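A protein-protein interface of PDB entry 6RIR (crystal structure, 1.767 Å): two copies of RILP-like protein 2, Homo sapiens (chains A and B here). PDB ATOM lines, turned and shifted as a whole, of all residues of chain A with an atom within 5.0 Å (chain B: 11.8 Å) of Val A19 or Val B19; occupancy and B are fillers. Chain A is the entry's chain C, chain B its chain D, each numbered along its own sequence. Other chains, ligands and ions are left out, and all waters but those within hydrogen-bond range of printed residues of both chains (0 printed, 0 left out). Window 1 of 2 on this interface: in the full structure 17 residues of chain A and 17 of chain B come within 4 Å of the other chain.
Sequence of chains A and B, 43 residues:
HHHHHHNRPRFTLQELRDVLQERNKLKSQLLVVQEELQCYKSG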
ATOM      1  N   GLU A  15       8.122   1.970  26.317  1.00  0.00           N
ATOM      2  CA  GLU A  15       7.278   2.581  27.350  1.00  0.00           C
ATOM      3  C   GLU A  15       6.798   3.965  26.929  1.00  0.00           C
ATOM      4  O   GLU A  15       5.609   4.280  27.029  1.00  0.00           O
ATOM      5  CB  GLU A  15       8.048   2.645  28.672  1.00  0.00           C
ATOM      6  CG  GLU A  15       8.238   1.255  29.308  1.00  0.00           C
ATOM      7  CD  GLU A  15       9.113   1.277  30.555  1.00  0.00           C
ATOM      8  OE1 GLU A  15      10.111   2.023  30.577  1.00  0.00           O
ATOM      9  OE2 GLU A  15       8.806   0.545  31.516  1.00  0.00           O
ATOM     10  N   LEU A  16       7.707   4.809  26.443  1.00  0.00           N
ATOM     11  CA  LEU A  16       7.299   6.147  26.019  1.00  0.00           C
ATOM     12  C   LEU A  16       6.404   6.087  24.785  1.00  0.00           C
ATOM     13  O   LEU A  16       5.398   6.800  24.702  1.00  0.00           O
ATOM     14  CB  LEU A  16       8.532   7.005  25.750  1.00  0.00           C
ATOM     15  CG  LEU A  16       8.203   8.425  25.284  1.00  0.00           C
ATOM     16  CD1 LEU A  16       7.663   9.241  26.453  1.00  0.00           C
ATOM     17  CD2 LEU A  16       9.432   9.093  24.677  1.00  0.00           C
ATOM     18  N   ARG A  17       6.738   5.216  23.839  1.00  0.00           N
ATOM     19  CA  ARG A  17       5.957   5.111  22.609  1.00  0.00           C
ATOM     20  C   ARG A  17       4.524   4.666  22.899  1.00  0.00           C
ATOM     21  O   ARG A  17       3.569   5.210  22.326  1.00  0.00           O
ATOM     22  CB  ARG A  17       6.676   4.150  21.665  1.00  0.00           C
ATOM     23  CG  ARG A  17       5.874   3.558  20.544  1.00  0.00           C
ATOM     24  CD  ARG A  17       6.755   2.560  19.810  1.00  0.00           C
ATOM     25  NE  ARG A  17       7.322   3.154  18.604  1.00  0.00           N
ATOM     26  CZ  ARG A  17       8.370   2.666  17.944  1.00  0.00           C
ATOM     27  NH1 ARG A  17       8.981   1.569  18.376  1.00  0.00           N
ATOM     28  NH2 ARG A  17       8.803   3.282  16.852  1.00  0.00           N
ATOM     29  N   ASP A  18       4.350   3.702  23.814  1.00  0.00           N
ATOM     30  CA  ASP A  18       3.004   3.227  24.135  1.00  0.00           C
ATOM     31  C   ASP A  18       2.140   4.348  24.703  1.00  0.00           C
ATOM     32  O   ASP A  18       0.957   4.461  24.357  1.00  0.00           O
ATOM     33  CB  ASP A  18       3.065   2.064  25.131  1.00  0.00           C
ATOM     34  CG  ASP A  18       3.511   0.744  24.492  1.00  0.00           C
ATOM     35  OD1 ASP A  18       3.726   0.696  23.255  1.00  0.00           O
ATOM     36  OD2 ASP A  18       3.648  -0.252  25.242  1.00  0.00           O
ATOM     37  N   VAL A  19       2.702   5.170  25.599  1.00  0.00           N
ATOM     38  CA  VAL A  19       1.917   6.247  26.206  1.00  0.00           C
ATOM     39  C   VAL A  19       1.653   7.359  25.196  1.00  0.00           C
ATOM     40  O   VAL A  19       0.587   7.985  25.215  1.00  0.00           O
ATOM     41  CB  VAL A  19       2.606   6.806  27.468  1.00  0.00           C
ATOM     42  CG1 VAL A  19       1.707   7.849  28.131  1.00  0.00           C
ATOM     43  CG2 VAL A  19       2.907   5.699  28.462  1.00  0.00           C
ATOM     44  N   LEU A  20       2.624   7.649  24.320  1.00  0.00           N
ATOM     45  CA  LEU A  20       2.367   8.609  23.245  1.00  0.00           C
ATOM     46  C   LEU A  20       1.233   8.127  22.351  1.00  0.00           C
ATOM     47  O   LEU A  20       0.316   8.892  22.024  1.00  0.00           O
ATOM     48  CB  LEU A  20       3.631   8.843  22.408  1.00  0.00           C
ATOM     49  CG  LEU A  20       4.710   9.775  22.959  1.00  0.00           C
ATOM     50  CD1 LEU A  20       6.026   9.579  22.190  1.00  0.00           C
ATOM     51  CD2 LEU A  20       4.258  11.241  22.922  1.00  0.00           C
ATOM     52  N   GLN A  21       1.292   6.857  21.931  1.00  0.00           N
ATOM     53  CA  GLN A  21       0.239   6.303  21.086  1.00  0.00           C
ATOM     54  C   GLN A  21      -1.115   6.396  21.769  1.00  0.00           C
ATOM     55  O   GLN A  21      -2.116   6.753  21.137  1.00  0.00           O
ATOM     56  CB  GLN A  21       0.559   4.849  20.718  1.00  0.00           C
ATOM     57  CG  GLN A  21       1.693   4.708  19.692  1.00  0.00           C
ATOM     58  CD  GLN A  21       2.178   3.279  19.514  1.00  0.00           C
ATOM     59  OE1 GLN A  21       1.657   2.346  20.126  1.00  0.00           O
ATOM     60  NE2 GLN A  21       3.182   3.100  18.654  1.00  0.00           N
ATOM     61  N   GLU A  22      -1.166   6.096  23.070  1.00  0.00           N
ATOM     62  CA  GLU A  22      -2.429   6.201  23.791  1.00  0.00           C
ATOM     63  C   GLU A  22      -2.905   7.644  23.847  1.00  0.00           C
ATOM     64  O   GLU A  22      -4.087   7.922  23.614  1.00  0.00           O
ATOM     65  CB  GLU A  22      -2.281   5.606  25.193  1.00  0.00           C
ATOM     66  CG  GLU A  22      -2.170   4.085  25.159  1.00  0.00           C
ATOM     67  CD  GLU A  22      -1.256   3.498  26.230  1.00  0.00           C
ATOM     68  OE1 GLU A  22      -0.912   4.208  27.202  1.00  0.00           O
ATOM     69  OE2 GLU A  22      -0.888   2.309  26.092  1.00  0.00           O
ATOM     70  N   ARG A  23      -1.999   8.583  24.140  1.00  0.00           N
ATOM     71  CA  ARG A  23      -2.369   9.997  24.162  1.00  0.00           C
ATOM     72  C   ARG A  23      -2.932  10.443  22.815  1.00  0.00           C
ATOM     73  O   ARG A  23      -3.983  11.090  22.745  1.00  0.00           O
ATOM     74  CB  ARG A  23      -1.155  10.851  24.538  1.00  0.00           C
ATOM     75  CG  ARG A  23      -1.501  12.305  24.854  1.00  0.00           C
ATOM     76  CD  ARG A  23      -0.310  13.232  24.640  1.00  0.00           C
ATOM     77  NE  ARG A  23       0.161  13.160  23.256  1.00  0.00           N
ATOM     78  CZ  ARG A  23       1.352  13.579  22.843  1.00  0.00           C
ATOM     79  NH1 ARG A  23       2.217  14.106  23.705  1.00  0.00           N
ATOM     80  NH2 ARG A  23       1.682  13.449  21.563  1.00  0.00           N
ATOM     81  N   ASN A  24      -2.244  10.108  21.729  1.00  0.00           N
ATOM     82  CA  ASN A  24      -2.717  10.576  20.433  1.00  0.00           C
ATOM     83  C   ASN A  24      -4.062   9.953  20.076  1.00  0.00           C
ATOM     84  O   ASN A  24      -4.942  10.639  19.548  1.00  0.00           O
ATOM     85  CB  ASN A  24      -1.668  10.300  19.357  1.00  0.00           C
ATOM     86  CG  ASN A  24      -0.377  11.056  19.600  1.00  0.00           C
ATOM     87  OD1 ASN A  24      -0.355  12.095  20.277  1.00  0.00           O
ATOM     88  ND2 ASN A  24       0.717  10.525  19.072  1.00  0.00           N
ATOM     89  N   PHE B  11      14.535   7.414  28.307  1.00  0.00           N
ATOM     90  CA  PHE B  11      13.795   8.650  28.513  1.00  0.00           C
ATOM     91  C   PHE B  11      13.639   8.965  29.997  1.00  0.00           C
ATOM     92  O   PHE B  11      13.621   8.072  30.852  1.00  0.00           O
ATOM     93  CB  PHE B  11      12.444   8.577  27.787  1.00  0.00           C
ATOM     94  CG  PHE B  11      12.601   8.294  26.326  1.00  0.00           C
ATOM     95  CD1 PHE B  11      12.964   9.311  25.449  1.00  0.00           C
ATOM     96  CD2 PHE B  11      12.455   7.005  25.831  1.00  0.00           C
ATOM     97  CE1 PHE B  11      13.144   9.055  24.104  1.00  0.00           C
ATOM     98  CE2 PHE B  11      12.639   6.736  24.486  1.00  0.00           C
ATOM     99  CZ  PHE B  11      12.983   7.771  23.618  1.00  0.00           C
ATOM    100  N   THR B  12      13.559  10.259  30.294  1.00  0.00           N
ATOM    101  CA  THR B  12      13.613  10.760  31.658  1.00  0.00           C
ATOM    102  C   THR B  12      12.254  10.654  32.336  1.00  0.00           C
ATOM    103  O   THR B  12      11.216  10.468  31.697  1.00  0.00           O
ATOM    104  CB  THR B  12      14.050  12.227  31.680  1.00  0.00           C
ATOM    105  OG1 THR B  12      13.012  13.027  31.090  1.00  0.00           O
ATOM    106  CG2 THR B  12      15.340  12.415  30.901  1.00  0.00           C
ATOM    107  N   LEU B  13      12.269  10.843  33.655  1.00  0.00           N
ATOM    108  CA  LEU B  13      11.022  10.890  34.415  1.00  0.00           C
ATOM    109  C   LEU B  13      10.104  11.998  33.900  1.00  0.00           C
ATOM    110  O   LEU B  13       8.905  11.783  33.677  1.00  0.00           O
ATOM    111  CB  LEU B  13      11.349  11.082  35.892  1.00  0.00           C
ATOM    112  CG  LEU B  13      10.222  11.258  36.903  1.00  0.00           C
ATOM    113  CD1 LEU B  13       9.288  10.062  36.870  1.00  0.00           C
ATOM    114  CD2 LEU B  13      10.818  11.460  38.287  1.00  0.00           C
ATOM    115  N   GLN B  14      10.662  13.188  33.670  1.00  0.00           N
ATOM    116  CA  GLN B  14       9.836  14.307  33.222  1.00  0.00           C
ATOM    117  C   GLN B  14       9.249  14.051  31.837  1.00  0.00           C
ATOM    118  O   GLN B  14       8.094  14.405  31.570  1.00  0.00           O
ATOM    119  CB  GLN B  14      10.650  15.603  33.245  1.00  0.00           C
ATOM    120  CG  GLN B  14       9.791  16.878  33.244  1.00  0.00           C
ATOM    121  CD  GLN B  14       8.929  17.021  34.501  1.00  0.00           C
ATOM    122  OE1 GLN B  14       9.442  17.107  35.618  1.00  0.00           O
ATOM    123  NE2 GLN B  14       7.611  17.044  34.316  1.00  0.00           N
ATOM    124  N   GLU B  15      10.019  13.427  30.938  1.00  0.00           N
ATOM    125  CA  GLU B  15       9.495  13.129  29.610  1.00  0.00           C
ATOM    126  C   GLU B  15       8.305  12.178  29.691  1.00  0.00           C
ATOM    127  O   GLU B  15       7.279  12.388  29.036  1.00  0.00           O
ATOM    128  CB  GLU B  15      10.591  12.532  28.729  1.00  0.00           C
ATOM    129  CG  GLU B  15      11.631  13.543  28.225  1.00  0.00           C
ATOM    130  CD  GLU B  15      12.801  12.870  27.510  1.00  0.00           C
ATOM    131  OE1 GLU B  15      13.218  11.781  27.949  1.00  0.00           O
ATOM    132  OE2 GLU B  15      13.307  13.426  26.505  1.00  0.00           O
ATOM    133  N   LEU B  16       8.425  11.118  30.489  1.00  0.00           N
ATOM    134  CA  LEU B  16       7.331  10.159  30.575  1.00  0.00           C
ATOM    135  C   LEU B  16       6.149  10.746  31.330  1.00  0.00           C
ATOM    136  O   LEU B  16       4.994  10.607  30.900  1.00  0.00           O
ATOM    137  CB  LEU B  16       7.802   8.869  31.246  1.00  0.00           C
ATOM    138  CG  LEU B  16       6.717   7.782  31.205  1.00  0.00           C
ATOM    139  CD1 LEU B  16       6.631   7.181  29.825  1.00  0.00           C
ATOM    140  CD2 LEU B  16       7.001   6.700  32.253  1.00  0.00           C
ATOM    141  N   ARG B  17       6.425  11.422  32.445  1.00  0.00           N
ATOM    142  CA  ARG B  17       5.377  12.055  33.239  1.00  0.00           C
ATOM    143  C   ARG B  17       4.568  13.043  32.418  1.00  0.00           C
ATOM    144  O   ARG B  17       3.334  13.083  32.519  1.00  0.00           O
ATOM    145  CB  ARG B  17       6.000  12.778  34.425  1.00  0.00           C
ATOM    146  CG  ARG B  17       5.512  12.346  35.756  1.00  0.00           C
ATOM    147  CD  ARG B  17       6.307  13.081  36.800  1.00  0.00           C
ATOM    148  NE  ARG B  17       5.974  12.615  38.126  1.00  0.00           N
ATOM    149  CZ  ARG B  17       6.667  12.929  39.206  1.00  0.00           C
ATOM    150  NH1 ARG B  17       6.287  12.455  40.387  1.00  0.00           N
ATOM    151  NH2 ARG B  17       7.741  13.710  39.102  1.00  0.00           N
ATOM    152  N   ASP B  18       5.251  13.899  31.645  1.00  0.00           N
ATOM    153  CA  ASP B  18       4.538  14.873  30.819  1.00  0.00           C
ATOM    154  C   ASP B  18       3.517  14.187  29.912  1.00  0.00           C
ATOM    155  O   ASP B  18       2.373  14.637  29.800  1.00  0.00           O
ATOM    156  CB  ASP B  18       5.525  15.706  29.996  1.00  0.00           C
ATOM    157  CG  ASP B  18       6.249  16.776  30.834  1.00  0.00           C
ATOM    158  OD1 ASP B  18       5.940  16.928  32.039  1.00  0.00           O
ATOM    159  OD2 ASP B  18       7.135  17.468  30.281  1.00  0.00           O
ATOM    160  N   VAL B  19       3.903  13.081  29.269  1.00  0.00           N
ATOM    161  CA  VAL B  19       2.969  12.413  28.361  1.00  0.00           C
ATOM    162  C   VAL B  19       1.866  11.720  29.152  1.00  0.00           C
ATOM    163  O   VAL B  19       0.682  11.794  28.795  1.00  0.00           O
ATOM    164  CB  VAL B  19       3.717  11.429  27.439  1.00  0.00           C
ATOM    165  CG1 VAL B  19       2.747  10.783  26.420  1.00  0.00           C
ATOM    166  CG2 VAL B  19       4.863  12.141  26.720  1.00  0.00           C
ATOM    167  N   LEU B  20       2.232  11.059  30.252  1.00  0.00           N
ATOM    168  CA  LEU B  20       1.233  10.425  31.110  1.00  0.00           C
ATOM    169  C   LEU B  20       0.192  11.427  31.582  1.00  0.00           C
ATOM    170  O   LEU B  20      -1.015  11.152  31.533  1.00  0.00           O
ATOM    171  CB  LEU B  20       1.911   9.774  32.319  1.00  0.00           C
ATOM    172  CG  LEU B  20       2.461   8.369  32.158  1.00  0.00           C
ATOM    173  CD1 LEU B  20       3.203   7.982  33.445  1.00  0.00           C
ATOM    174  CD2 LEU B  20       1.335   7.399  31.846  1.00  0.00           C
ATOM    175  N   GLN B  21       0.634  12.599  32.042  1.00  0.00           N
ATOM    176  CA  GLN B  21      -0.320  13.589  32.537  1.00  0.00           C
ATOM    177  C   GLN B  21      -1.171  14.171  31.407  1.00  0.00           C
ATOM    178  O   GLN B  21      -2.360  14.459  31.605  1.00  0.00           O
ATOM    179  CB  GLN B  21       0.412  14.689  33.299  1.00  0.00           C
ATOM    180  CG  GLN B  21       0.902  14.216  34.681  1.00  0.00           C
ATOM    181  CD  GLN B  21       1.982  15.105  35.275  1.00  0.00           C
ATOM    182  OE1 GLN B  21       2.279  16.184  34.751  1.00  0.00           O
ATOM    183  NE2 GLN B  21       2.585  14.649  36.370  1.00  0.00           N
ATOM    184  N   GLU B  22      -0.587  14.363  30.222  1.00  0.00           N
ATOM    185  CA  GLU B  22      -1.408  14.751  29.074  1.00  0.00           C
ATOM    186  C   GLU B  22      -2.442  13.673  28.757  1.00  0.00           C
ATOM    187  O   GLU B  22      -3.613  13.979  28.490  1.00  0.00           O
ATOM    188  CB  GLU B  22      -0.519  15.021  27.853  1.00  0.00           C
ATOM    189  CG  GLU B  22       0.313  16.303  27.961  1.00  0.00           C
ATOM    190  CD  GLU B  22       1.649  16.241  27.214  1.00  0.00           C
ATOM    191  OE1 GLU B  22       2.434  17.211  27.325  1.00  0.00           O
ATOM    192  OE2 GLU B  22       1.919  15.239  26.517  1.00  0.00           O
ATOM    193  N   ARG B  23      -2.023  12.405  28.787  1.00  0.00           N
ATOM    194  CA  ARG B  23      -2.933  11.295  28.527  1.00  0.00           C
ATOM    195  C   ARG B  23      -4.067  11.267  29.539  1.00  0.00           C
ATOM    196  O   ARG B  23      -5.240  11.116  29.170  1.00  0.00           O
ATOM    197  CB  ARG B  23      -2.174   9.966  28.554  1.00  0.00           C
ATOM    198  CG  ARG B  23      -2.922   8.878  27.803  1.00  0.00           C
ATOM    199  CD  ARG B  23      -2.651   7.496  28.312  1.00  0.00           C
ATOM    200  NE  ARG B  23      -2.775   7.424  29.759  1.00  0.00           N
ATOM    201  CZ  ARG B  23      -2.187   6.488  30.490  1.00  0.00           C
ATOM    202  NH1 ARG B  23      -1.448   5.562  29.896  1.00  0.00           N
ATOM    203  NH2 ARG B  23      -2.325   6.489  31.803  1.00  0.00           N
ATOM    204  N   ASN B  24      -3.732  11.408  30.826  1.00  0.00           N
ATOM    205  CA  ASN B  24      -4.761  11.437  31.862  1.00  0.00           C
ATOM    206  C   ASN B  24      -5.743  12.572  31.630  1.00  0.00           C
ATOM    207  O   ASN B  24      -6.960  12.389  31.765  1.00  0.00           O
ATOM    208  CB  ASN B  24      -4.135  11.604  33.248  1.00  0.00           C
ATOM    209  CG  ASN B  24      -3.372  10.393  33.702  1.00  0.00           C
ATOM    210  OD1 ASN B  24      -3.457   9.310  33.113  1.00  0.00           O
ATOM    211  ND2 ASN B  24      -2.593  10.573  34.765  1.00  0.00           N
ATOM    212  N   LYS B  25      -5.230  13.760  31.297  1.00  0.00           N
ATOM    213  CA  LYS B  25      -6.109  14.911  31.117  1.00  0.00           C
ATOM    214  C   LYS B  25      -7.085  14.685  29.966  1.00  0.00           C
ATOM    215  O   LYS B  25      -8.278  14.981  30.094  1.00  0.00           O
ATOM    216  CB  LYS B  25      -5.282  16.177  30.880  1.00  0.00           C
ATOM    217  CG  LYS B  25      -6.118  17.424  30.736  1.00  0.00           C
ATOM    218  CD  LYS B  25      -5.264  18.638  30.425  1.00  0.00           C
ATOM    219  CE  LYS B  25      -6.143  19.849  30.163  1.00  0.00           C
ATOM    220  NZ  LYS B  25      -7.250  19.955  31.161  1.00  0.00           N
ATOM    221  N   LEU B  26      -6.597  14.155  28.836  1.00  0.00           N
ATOM    222  CA  LEU B  26      -7.465  13.895  27.691  1.00  0.00           C
ATOM    223  C   LEU B  26      -8.513  12.837  28.012  1.00  0.00           C
ATOM    224  O   LEU B  26      -9.657  12.924  27.552  1.00  0.00           O
ATOM    225  CB  LEU B  26      -6.628  13.459  26.488  1.00  0.00           C
ATOM    226  CG  LEU B  26      -5.777  14.560  25.842  1.00  0.00           C
ATOM    227  CD1 LEU B  26      -4.691  13.937  25.004  1.00  0.00           C
ATOM    228  CD2 LEU B  26      -6.649  15.482  24.986  1.00  0.00           C
ATOM    229  N   LYS B  27      -8.140  11.822  28.792  1.00  0.00           N
ATOM    230  CA  LYS B  27      -9.123  10.812  29.177  1.00  0.00           C
ATOM    231  C   LYS B  27     -10.245  11.436  29.994  1.00  0.00           C
ATOM    232  O   LYS B  27     -11.426  11.150  29.764  1.00  0.00           O
ATOM    233  CB  LYS B  27      -8.435   9.689  29.965  1.00  0.00           C
ATOM    234  CG  LYS B  27      -9.216   8.384  30.014  1.00  0.00           C
ATOM    235  CD  LYS B  27      -8.400   7.296  30.696  1.00  0.00           C
ATOM    236  CE  LYS B  27      -9.073   5.943  30.601  1.00  0.00           C
ATOM    237  NZ  LYS B  27      -8.164   4.855  31.066  1.00  0.00           N
ATOM    238  N   SER B  28      -9.894  12.287  30.959  1.00  0.00           N
ATOM    239  CA  SER B  28     -10.907  12.966  31.754  1.00  0.00           C
ATOM    240  C   SER B  28     -11.798  13.834  30.880  1.00  0.00           C
ATOM    241  O   SER B  28     -13.029  13.811  31.011  1.00  0.00           O
ATOM    242  CB  SER B  28     -10.237  13.814  32.837  1.00  0.00           C
ATOM    243  OG  SER B  28      -9.734  12.982  33.869  1.00  0.00           O
ATOM    244  N   GLN B  29     -11.189  14.623  29.988  1.00  0.00           N
ATOM    245  CA  GLN B  29     -11.967  15.457  29.075  1.00  0.00           C
ATOM    246  C   GLN B  29     -12.869  14.613  28.180  1.00  0.00           C
ATOM    247  O   GLN B  29     -14.021  14.985  27.927  1.00  0.00           O
ATOM    248  CB  GLN B  29     -11.032  16.322  28.228  1.00  0.00           C
ATOM    249  CG  GLN B  29     -10.308  17.392  29.024  1.00  0.00           C
ATOM    250  CD  GLN B  29      -9.259  18.116  28.205  1.00  0.00           C
ATOM    251  OE1 GLN B  29      -8.592  17.518  27.359  1.00  0.00           O
ATOM    252  NE2 GLN B  29      -9.104  19.406  28.456  1.00  0.00           N
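The side-chain carboxylate of Glu B22 is in salt-bridge range of the guanidinium group of Arg A23 (3.0 Å).
The side-chain carboxylate of Glu A22 lies within salt-bridge range of the guanidinium group of Arg B23 (3.1 Å).
The backbone carbonyl oxygen of Leu B20 sits close to the side-chain amide oxygen of Asn B24 (3.4 Å).
The side-chain amide oxygen (OD1) of Asn B24 sits at hydrogen-bond distance from the guanidinium group (NH2) of Arg B23 (3.3 Å).
The backbone carbonyl oxygen (O) of Leu A20 sits close to the side-chain amide nitrogen (ND2) of Asn A24 (3.4 Å).
The guanidinium group of Arg A23 sits at hydrogen-bond distance from the side-chain amide oxygen of Asn A24, at 2.8 Å.
CD1 of Phe B11 touches CD2 of Leu A16 (3.6 Å).
Val A19 touches Val B19.
CG1 of Val A19 touches CD2 of Leu B20 (3.8 Å).
Leu A20 touches Val B19.
Arg A23 touches Arg B23 (N to CG, 3.8 Å).
Arg A23 touches Leu B26.
Val A19 touches just these residues of chain B: Val B19 and Leu B20.
Of chain A, only Val A19 (3.6 Å) and Leu A20 (3.8 Å) come within 4 Å of Val B19.
No residue of chain B comes within 4 Å of Asp A18.
Leu A20 touches just one residue of chain B: Val B19.
Of the printed residues of chain B, Glu A22 touches Arg B23 (3.1 Å).
Arg A23 touches just these residues of chain B: Glu B22 (3.0 Å), Arg B23 (3.8 Å) and Leu B26 (3.6 Å).
Printed residues of chain B within 4 Å of Leu A16: Phe B11 (3.6 Å).
Printed residues of chain A within 4 Å of Leu B26: Arg A23 (3.6 Å).
Printed residues of chain A within 4 Å of Arg B23: Glu A22 (3.1 Å) and Arg A23 (3.8 Å).
Gln B21 touches none of the printed residues of chain A.
Asn B24 touches none of the printed residues of chain A.
The nearest residue of chain B that does not touch Val A19 is Leu B16 (4.2 Å).
Hydrophobic or aromatic side chains of chain B that line the printed part of chain A: Phe B11, Val B19, Leu B20 and Leu B26.
Along chain B the printed residues that touch a printed residue of chain A span positions 11 to 26.
Among the printed residues, Asp or Glu carboxylates within 4 Å of a Lys or Arg side-chain nitrogen of the other chain: Glu A22 with Arg B23 (3.1 Å) and Arg A23 with Glu B22 (3.0 Å).
Val A19 touches its own counterpart, Val B19.
Val A19 touches Leu B20, and with the chains exchanged Leu A20 touches Val B19.
Glu A22 touches Arg B23, and with the chains exchanged Arg A23 touches Glu B22.
Arg B23 touches its own counterpart, Arg A23.
Of the 8 pairs that touch across the chains among the printed residues, 6 have their exchanged pair printed and touching as well.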
